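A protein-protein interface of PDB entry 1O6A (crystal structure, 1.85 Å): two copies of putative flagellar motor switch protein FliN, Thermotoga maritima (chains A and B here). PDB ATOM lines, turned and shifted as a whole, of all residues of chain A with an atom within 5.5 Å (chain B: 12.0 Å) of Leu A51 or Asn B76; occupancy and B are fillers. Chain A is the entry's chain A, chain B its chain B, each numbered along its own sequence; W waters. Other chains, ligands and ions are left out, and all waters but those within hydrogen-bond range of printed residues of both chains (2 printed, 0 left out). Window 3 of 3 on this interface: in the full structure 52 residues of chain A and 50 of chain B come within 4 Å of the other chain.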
ATOM      1  N   GLU A  47       8.680 -12.317   3.017  1.00  0.00           N
ATOM      2  CA  GLU A  47       9.812 -12.011   2.122  1.00  0.00           C
ATOM      3  C   GLU A  47      10.329 -13.294   1.498  1.00  0.00           C
ATOM      4  O   GLU A  47      10.411 -14.356   2.142  1.00  0.00           O
ATOM      5  CB  GLU A  47      10.896 -11.298   2.914  1.00  0.00           C
ATOM      6  CG  GLU A  47      12.034 -10.784   2.084  1.00  0.00           C
ATOM      7  CD  GLU A  47      12.999  -9.955   2.934  1.00  0.00           C
ATOM      8  OE1 GLU A  47      12.558  -9.374   3.977  1.00  0.00           O
ATOM      9  OE2 GLU A  47      14.184  -9.909   2.561  1.00  0.00           O
ATOM     10  N   LEU A  48      10.661 -13.221   0.212  1.00  0.00           N
ATOM     11  CA  LEU A  48      11.099 -14.368  -0.540  1.00  0.00           C
ATOM     12  C   LEU A  48      12.596 -14.287  -0.923  1.00  0.00           C
ATOM     13  O   LEU A  48      13.242 -13.240  -0.825  1.00  0.00           O
ATOM     14  CB  LEU A  48      10.266 -14.481  -1.804  1.00  0.00           C
ATOM     15  CG  LEU A  48       8.758 -14.557  -1.623  1.00  0.00           C
ATOM     16  CD1 LEU A  48       8.101 -14.367  -3.020  1.00  0.00           C
ATOM     17  CD2 LEU A  48       8.389 -15.848  -0.951  1.00  0.00           C
ATOM     18  N   ASP A  49      13.118 -15.425  -1.342  1.00  0.00           N
ATOM     19  CA  ASP A  49      14.509 -15.594  -1.664  1.00  0.00           C
ATOM     20  C   ASP A  49      14.897 -15.043  -3.020  1.00  0.00           C
ATOM     21  O   ASP A  49      16.043 -15.083  -3.365  1.00  0.00           O
ATOM     22  CB  ASP A  49      14.927 -17.090  -1.527  1.00  0.00           C
ATOM     23  CG  ASP A  49      14.235 -18.070  -2.571  1.00  0.00           C
ATOM     24  OD1 ASP A  49      13.413 -17.697  -3.481  1.00  0.00           O
ATOM     25  OD2 ASP A  49      14.501 -19.317  -2.523  1.00  0.00           O
ATOM     26  N   LYS A  50      13.981 -14.419  -3.713  1.00  0.00           N
ATOM     27  CA  LYS A  50      14.247 -13.842  -5.030  1.00  0.00           C
ATOM     28  C   LYS A  50      14.582 -12.338  -4.956  1.00  0.00           C
ATOM     29  O   LYS A  50      13.959 -11.580  -4.226  1.00  0.00           O
ATOM     30  CB  LYS A  50      13.032 -14.096  -5.910  1.00  0.00           C
ATOM     31  CG  LYS A  50      13.312 -13.800  -7.435  1.00  0.00           C
ATOM     32  CD  LYS A  50      12.144 -14.150  -8.373  1.00  0.00           C
ATOM     33  CE  LYS A  50      11.964 -15.682  -8.508  1.00  0.00           C
ATOM     34  NZ  LYS A  50      13.165 -16.353  -9.024  1.00  0.00           N
ATOM     35  N   LEU A  51      15.607 -11.929  -5.698  1.00  0.00           N
ATOM     36  CA  LEU A  51      16.060 -10.565  -5.717  1.00  0.00           C
ATOM     37  C   LEU A  51      15.461  -9.800  -6.878  1.00  0.00           C
ATOM     38  O   LEU A  51      15.233 -10.341  -7.949  1.00  0.00           O
ATOM     39  CB  LEU A  51      17.614 -10.482  -5.799  1.00  0.00           C
ATOM     40  CG  LEU A  51      18.376 -11.225  -4.688  1.00  0.00           C
ATOM     41  CD1 LEU A  51      19.839 -11.486  -5.043  1.00  0.00           C
ATOM     42  CD2 LEU A  51      18.282 -10.525  -3.385  1.00  0.00           C
ATOM     43  N   THR A  52      15.312  -8.491  -6.686  1.00  0.00           N
ATOM     44  CA  THR A  52      14.907  -7.642  -7.794  1.00  0.00           C
ATOM     45  C   THR A  52      16.055  -7.681  -8.810  1.00  0.00           C
ATOM     46  O   THR A  52      17.272  -7.673  -8.486  1.00  0.00           O
ATOM     47  CB  THR A  52      14.584  -6.199  -7.373  1.00  0.00           C
ATOM     48  OG1 THR A  52      15.689  -5.646  -6.666  1.00  0.00           O
ATOM     49  CG2 THR A  52      13.416  -6.166  -6.405  1.00  0.00           C
ATOM     50  N   GLY A  53      15.670  -7.753 -10.053  1.00  0.00           N
ATOM     51  CA  GLY A  53      16.637  -7.979 -11.094  1.00  0.00           C
ATOM     52  C   GLY A  53      16.687  -9.425 -11.546  1.00  0.00           C
ATOM     53  O   GLY A  53      17.287  -9.696 -12.577  1.00  0.00           O
ATOM     54  N   GLU A  54      16.056 -10.344 -10.805  1.00  0.00           N
ATOM     55  CA  GLU A  54      16.024 -11.751 -11.223  1.00  0.00           C
ATOM     56  C   GLU A  54      14.736 -12.118 -11.911  1.00  0.00           C
ATOM     57  O   GLU A  54      13.689 -11.520 -11.638  1.00  0.00           O
ATOM     58  CB  GLU A  54      16.209 -12.671 -10.057  1.00  0.00           C
ATOM     59  CG  GLU A  54      17.559 -12.566  -9.380  1.00  0.00           C
ATOM     60  CD  GLU A  54      17.771 -13.739  -8.448  1.00  0.00           C
ATOM     61  OE1 GLU A  54      17.125 -13.737  -7.374  1.00  0.00           O
ATOM     62  OE2 GLU A  54      18.563 -14.657  -8.777  1.00  0.00           O
ATOM     63  N   VAL B  25       5.450 -18.935  -3.670  1.00  0.00           N
ATOM     64  CA  VAL B  25       4.519 -17.982  -4.219  1.00  0.00           C
ATOM     65  C   VAL B  25       4.483 -18.219  -5.722  1.00  0.00           C
ATOM     66  O   VAL B  25       5.528 -18.171  -6.403  1.00  0.00           O
ATOM     67  CB  VAL B  25       4.936 -16.558  -3.892  1.00  0.00           C
ATOM     68  CG1 VAL B  25       4.020 -15.544  -4.561  1.00  0.00           C
ATOM     69  CG2 VAL B  25       4.894 -16.367  -2.368  1.00  0.00           C
ATOM     70  N   GLU B  69      -0.492  -9.698  -2.793  1.00  0.00           N
ATOM     71  CA  GLU B  69       0.053  -8.761  -3.765  1.00  0.00           C
ATOM     72  C   GLU B  69       1.574  -8.718  -3.651  1.00  0.00           C
ATOM     73  O   GLU B  69       2.116  -8.767  -2.546  1.00  0.00           O
ATOM     74  CB  GLU B  69      -0.562  -7.375  -3.522  1.00  0.00           C
ATOM     75  CG  GLU B  69      -2.073  -7.370  -3.777  1.00  0.00           C
ATOM     76  CD  GLU B  69      -2.770  -6.036  -3.520  1.00  0.00           C
ATOM     77  OE1 GLU B  69      -2.260  -5.186  -2.747  1.00  0.00           O
ATOM     78  OE2 GLU B  69      -3.864  -5.856  -4.094  1.00  0.00           O
ATOM     79  N   VAL B  70       2.266  -8.618  -4.778  1.00  0.00           N
ATOM     80  CA  VAL B  70       3.715  -8.607  -4.754  1.00  0.00           C
ATOM     81  C   VAL B  70       4.203  -7.244  -4.287  1.00  0.00           C
ATOM     82  O   VAL B  70       3.656  -6.193  -4.643  1.00  0.00           O
ATOM     83  CB  VAL B  70       4.287  -8.967  -6.126  1.00  0.00           C
ATOM     84  CG1 VAL B  70       5.842  -8.897  -6.099  1.00  0.00           C
ATOM     85  CG2 VAL B  70       3.828 -10.341  -6.505  1.00  0.00           C
ATOM     86  N   VAL B  71       5.218  -7.265  -3.453  1.00  0.00           N
ATOM     87  CA  VAL B  71       5.884  -6.090  -2.970  1.00  0.00           C
ATOM     88  C   VAL B  71       7.376  -6.286  -3.079  1.00  0.00           C
ATOM     89  O   VAL B  71       7.872  -7.386  -3.258  1.00  0.00           O
ATOM     90  CB  VAL B  71       5.519  -5.746  -1.460  1.00  0.00           C
ATOM     91  CG1 VAL B  71       4.048  -5.406  -1.298  1.00  0.00           C
ATOM     92  CG2 VAL B  71       5.912  -6.870  -0.503  1.00  0.00           C
ATOM     93  N   VAL B  72       8.087  -5.193  -2.965  1.00  0.00           N
ATOM     94  CA  VAL B  72       9.546  -5.188  -2.818  1.00  0.00           C
ATOM     95  C   VAL B  72       9.934  -4.746  -1.435  1.00  0.00           C
ATOM     96  O   VAL B  72       9.469  -3.716  -0.975  1.00  0.00           O
ATOM     97  CB  VAL B  72      10.162  -4.246  -3.808  1.00  0.00           C
ATOM     98  CG1 VAL B  72      11.686  -4.146  -3.638  1.00  0.00           C
ATOM     99  CG2 VAL B  72       9.874  -4.730  -5.229  1.00  0.00           C
ATOM    100  N   ILE B  73      10.785  -5.516  -0.786  1.00  0.00           N
ATOM    101  CA  ILE B  73      11.351  -5.143   0.504  1.00  0.00           C
ATOM    102  C   ILE B  73      12.863  -5.069   0.309  1.00  0.00           C
ATOM    103  O   ILE B  73      13.532  -6.092   0.271  1.00  0.00           O
ATOM    104  CB  ILE B  73      10.990  -6.158   1.581  1.00  0.00           C
ATOM    105  CG1 ILE B  73       9.490  -6.446   1.635  1.00  0.00           C
ATOM    106  CG2 ILE B  73      11.475  -5.666   2.968  1.00  0.00           C
ATOM    107  CD1 ILE B  73       9.209  -7.898   1.604  1.00  0.00           C
ATOM    108  N   ASP B  74      13.331  -3.822   0.188  1.00  0.00           N
ATOM    109  CA  ASP B  74      14.732  -3.478  -0.053  1.00  0.00           C
ATOM    110  C   ASP B  74      15.108  -4.038  -1.429  1.00  0.00           C
ATOM    111  O   ASP B  74      14.708  -3.474  -2.441  1.00  0.00           O
ATOM    112  CB  ASP B  74      15.632  -3.975   1.101  1.00  0.00           C
ATOM    113  CG  ASP B  74      17.095  -3.574   0.949  1.00  0.00           C
ATOM    114  OD1 ASP B  74      17.429  -2.703   0.113  1.00  0.00           O
ATOM    115  OD2 ASP B  74      17.995  -4.104   1.643  1.00  0.00           O
ATOM    116  N   GLU B  75      15.840  -5.146  -1.485  1.00  0.00           N
ATOM    117  CA  GLU B  75      16.128  -5.757  -2.786  1.00  0.00           C
ATOM    118  C   GLU B  75      15.535  -7.153  -2.997  1.00  0.00           C
ATOM    119  O   GLU B  75      15.883  -7.800  -3.941  1.00  0.00           O
ATOM    120  CB  GLU B  75      17.618  -5.725  -3.104  1.00  0.00           C
ATOM    121  CG  GLU B  75      18.488  -6.598  -2.238  1.00  0.00           C
ATOM    122  CD  GLU B  75      19.935  -6.649  -2.691  1.00  0.00           C
ATOM    123  OE1 GLU B  75      20.363  -5.740  -3.463  1.00  0.00           O
ATOM    124  OE2 GLU B  75      20.658  -7.589  -2.231  1.00  0.00           O
ATOM    125  N   ASN B  76      14.618  -7.580  -2.152  1.00  0.00           N
ATOM    126  CA  ASN B  76      13.966  -8.882  -2.301  1.00  0.00           C
ATOM    127  C   ASN B  76      12.501  -8.694  -2.626  1.00  0.00           C
ATOM    128  O   ASN B  76      11.851  -7.751  -2.125  1.00  0.00           O
ATOM    129  CB  ASN B  76      14.078  -9.708  -1.013  1.00  0.00           C
ATOM    130  CG  ASN B  76      15.464 -10.282  -0.816  1.00  0.00           C
ATOM    131  OD1 ASN B  76      16.379  -9.532  -0.537  1.00  0.00           O
ATOM    132  ND2 ASN B  76      15.639 -11.607  -1.001  1.00  0.00           N
ATOM    133  N   PHE B  77      11.962  -9.607  -3.418  1.00  0.00           N
ATOM    134  CA  PHE B  77      10.527  -9.642  -3.591  1.00  0.00           C
ATOM    135  C   PHE B  77       9.878 -10.236  -2.359  1.00  0.00           C
ATOM    136  O   PHE B  77      10.489 -10.986  -1.588  1.00  0.00           O
ATOM    137  CB  PHE B  77      10.122 -10.472  -4.800  1.00  0.00           C
ATOM    138  CG  PHE B  77      10.415  -9.819  -6.083  1.00  0.00           C
ATOM    139  CD1 PHE B  77       9.642  -8.741  -6.531  1.00  0.00           C
ATOM    140  CD2 PHE B  77      11.505 -10.239  -6.856  1.00  0.00           C
ATOM    141  CE1 PHE B  77       9.934  -8.131  -7.699  1.00  0.00           C
ATOM    142  CE2 PHE B  77      11.783  -9.642  -8.032  1.00  0.00           C
ATOM    143  CZ  PHE B  77      11.021  -8.582  -8.466  1.00  0.00           C
ATOM    144  N   GLY B  78       8.624  -9.877  -2.194  1.00  0.00           N
ATOM    145  CA  GLY B  78       7.809 -10.360  -1.111  1.00  0.00           C
ATOM    146  C   GLY B  78       6.347 -10.348  -1.543  1.00  0.00           C
ATOM    147  O   GLY B  78       6.041  -9.929  -2.644  1.00  0.00           O
ATOM    148  N   VAL B  79       5.466 -10.814  -0.657  1.00  0.00           N
ATOM    149  CA  VAL B  79       4.027 -10.775  -0.879  1.00  0.00           C
ATOM    150  C   VAL B  79       3.369 -10.259   0.382  1.00  0.00           C
ATOM    151  O   VAL B  79       3.813 -10.582   1.492  1.00  0.00           O
ATOM    152  CB  VAL B  79       3.440 -12.147  -1.318  1.00  0.00           C
ATOM    153  CG1 VAL B  79       3.913 -12.469  -2.715  1.00  0.00           C
ATOM    154  CG2 VAL B  79       3.802 -13.262  -0.358  1.00  0.00           C
ATOM    155  N   ARG B  80       2.354  -9.423   0.199  1.00  0.00           N
ATOM    156  CA  ARG B  80       1.500  -8.937   1.278  1.00  0.00           C
ATOM    157  C   ARG B  80       0.179  -9.682   1.140  1.00  0.00           C
ATOM    158  O   ARG B  80      -0.474  -9.632   0.087  1.00  0.00           O
ATOM    159  CB  ARG B  80       1.309  -7.424   1.099  1.00  0.00           C
ATOM    160  CG  ARG B  80       0.442  -6.670   2.098  1.00  0.00           C
ATOM    161  CD  ARG B  80       0.362  -5.158   1.734  1.00  0.00           C
ATOM    162  NE  ARG B  80      -0.976  -4.586   1.762  1.00  0.00           N
ATOM    163  CZ  ARG B  80      -1.901  -4.726   0.807  1.00  0.00           C
ATOM    164  NH1 ARG B  80      -1.684  -5.452  -0.288  1.00  0.00           N
ATOM    165  NH2 ARG B  80      -3.078  -4.138   0.959  1.00  0.00           N
HETATM  166  O   HOH W   1      15.239  -3.344  -5.248  1.00  0.00           O
HETATM  167  O   HOH W   2      14.755  -7.303   2.338  1.00  0.00           O
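The side-chain amide nitrogen (ND2) of Asn B76 sits at hydrogen-bond distance from the backbone carbonyl oxygen (O) of Leu A48 (2.9 Å).
O of Phe B77 is in hydrogen-bond range of N of Leu A48.
The backbone NH of Phe B77 sits at hydrogen-bond distance from the backbone carbonyl oxygen of Lys A50 (2.9 Å).
The backbone NH (N) of Thr A52 lies within hydrogen-bond range of the backbone carbonyl oxygen (O) of Glu B75, 2.9 Å away.
The backbone NH of Leu A51 sits at hydrogen-bond distance from the side-chain carboxylate of Glu A54, at 2.9 Å.
Glu A47 touches Ile B73 (OE1 to CG2, 3.99 Å).
OE2 of Glu A47 touches CB of Asn B76 (3.6 Å).
Glu A47 touches Phe B77 (C to O, 3.9 Å).
Leu A48 touches Val B25 (CD2 to CG2, 3.8 Å).
Lys A50 touches Asn B76.
CA of Leu A51 touches O of Glu B75, 3.3 Å away.
Leu A51 touches Asn B76.
CE2 of Phe B77 touches O of Leu A51, 3.5 Å away.
CG2 of Thr A52 touches CG1 of Val B72, 3.8 Å away.
Thr A52 touches Phe B77 (CA to CE2, 3.7 Å).
Of the printed residues of chain B, Glu A47 touches Ile B73 (3.99 Å), Asn B76 (3.6 Å) and Phe B77 (3.9 Å).
No residue of chain B comes within 4 Å of Glu A54.
Val B70 touches none of the printed residues of chain A.
Printed residues of chain A within 4 Å of Val B72: Thr A52 (3.8 Å).
Printed residues of chain A within 4 Å of Ile B73: Glu A47.
Of the printed residues of chain A, Glu B75 touches Leu A51 (3.3 Å) and Thr A52 (2.9 Å).
Asn B76 touches just these residues of chain A: Glu A47, Leu A48, Lys A50 and Leu A51.
Printed residues of chain A within 4 Å of Phe B77: Glu A47, Leu A48, Lys A50, Leu A51 and Thr A52.
Val B79 touches none of the printed residues of chain A.
The nearest residue of chain A that does not touch Asn B76 is Asp A49 (4.1 Å).
Of the 8 printed residues of chain A, 5 touch a printed residue of chain B.
Hydrophobic or aromatic side chains of chain A within 4 Å of the printed part of chain B: Leu A48 and Leu A51.
Of the 13 printed residues of chain B, 6 touch a printed residue of chain A.
Printed residues of chain B that touch a printed residue of chain A: Val B25, Val B72, Ile B73, Glu B75, Asn B76 and Phe B77.
Among the printed residues, 14 pairs touch across the chains.
Among the printed residues, no Asp or Glu carboxylate lies within 4 Å of a Lys or Arg side-chain nitrogen of the other chain.
No position is printed for both chains.
Of the 14 pairs that touch across the chains among the printed residues, none has its exchanged pair printed and touching as well.
Water W2 lies within hydrogen-bond range of the side-chain carboxylate (OE2) of Glu A47 and the backbone carbonyl oxygen (O) of Ile B73.
Water W1 bridges the side-chain hydroxyl (OG1) of Thr A52 (2.7 Å) and the backbone carbonyl oxygen (O) of Asp B74 (2.9 Å).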
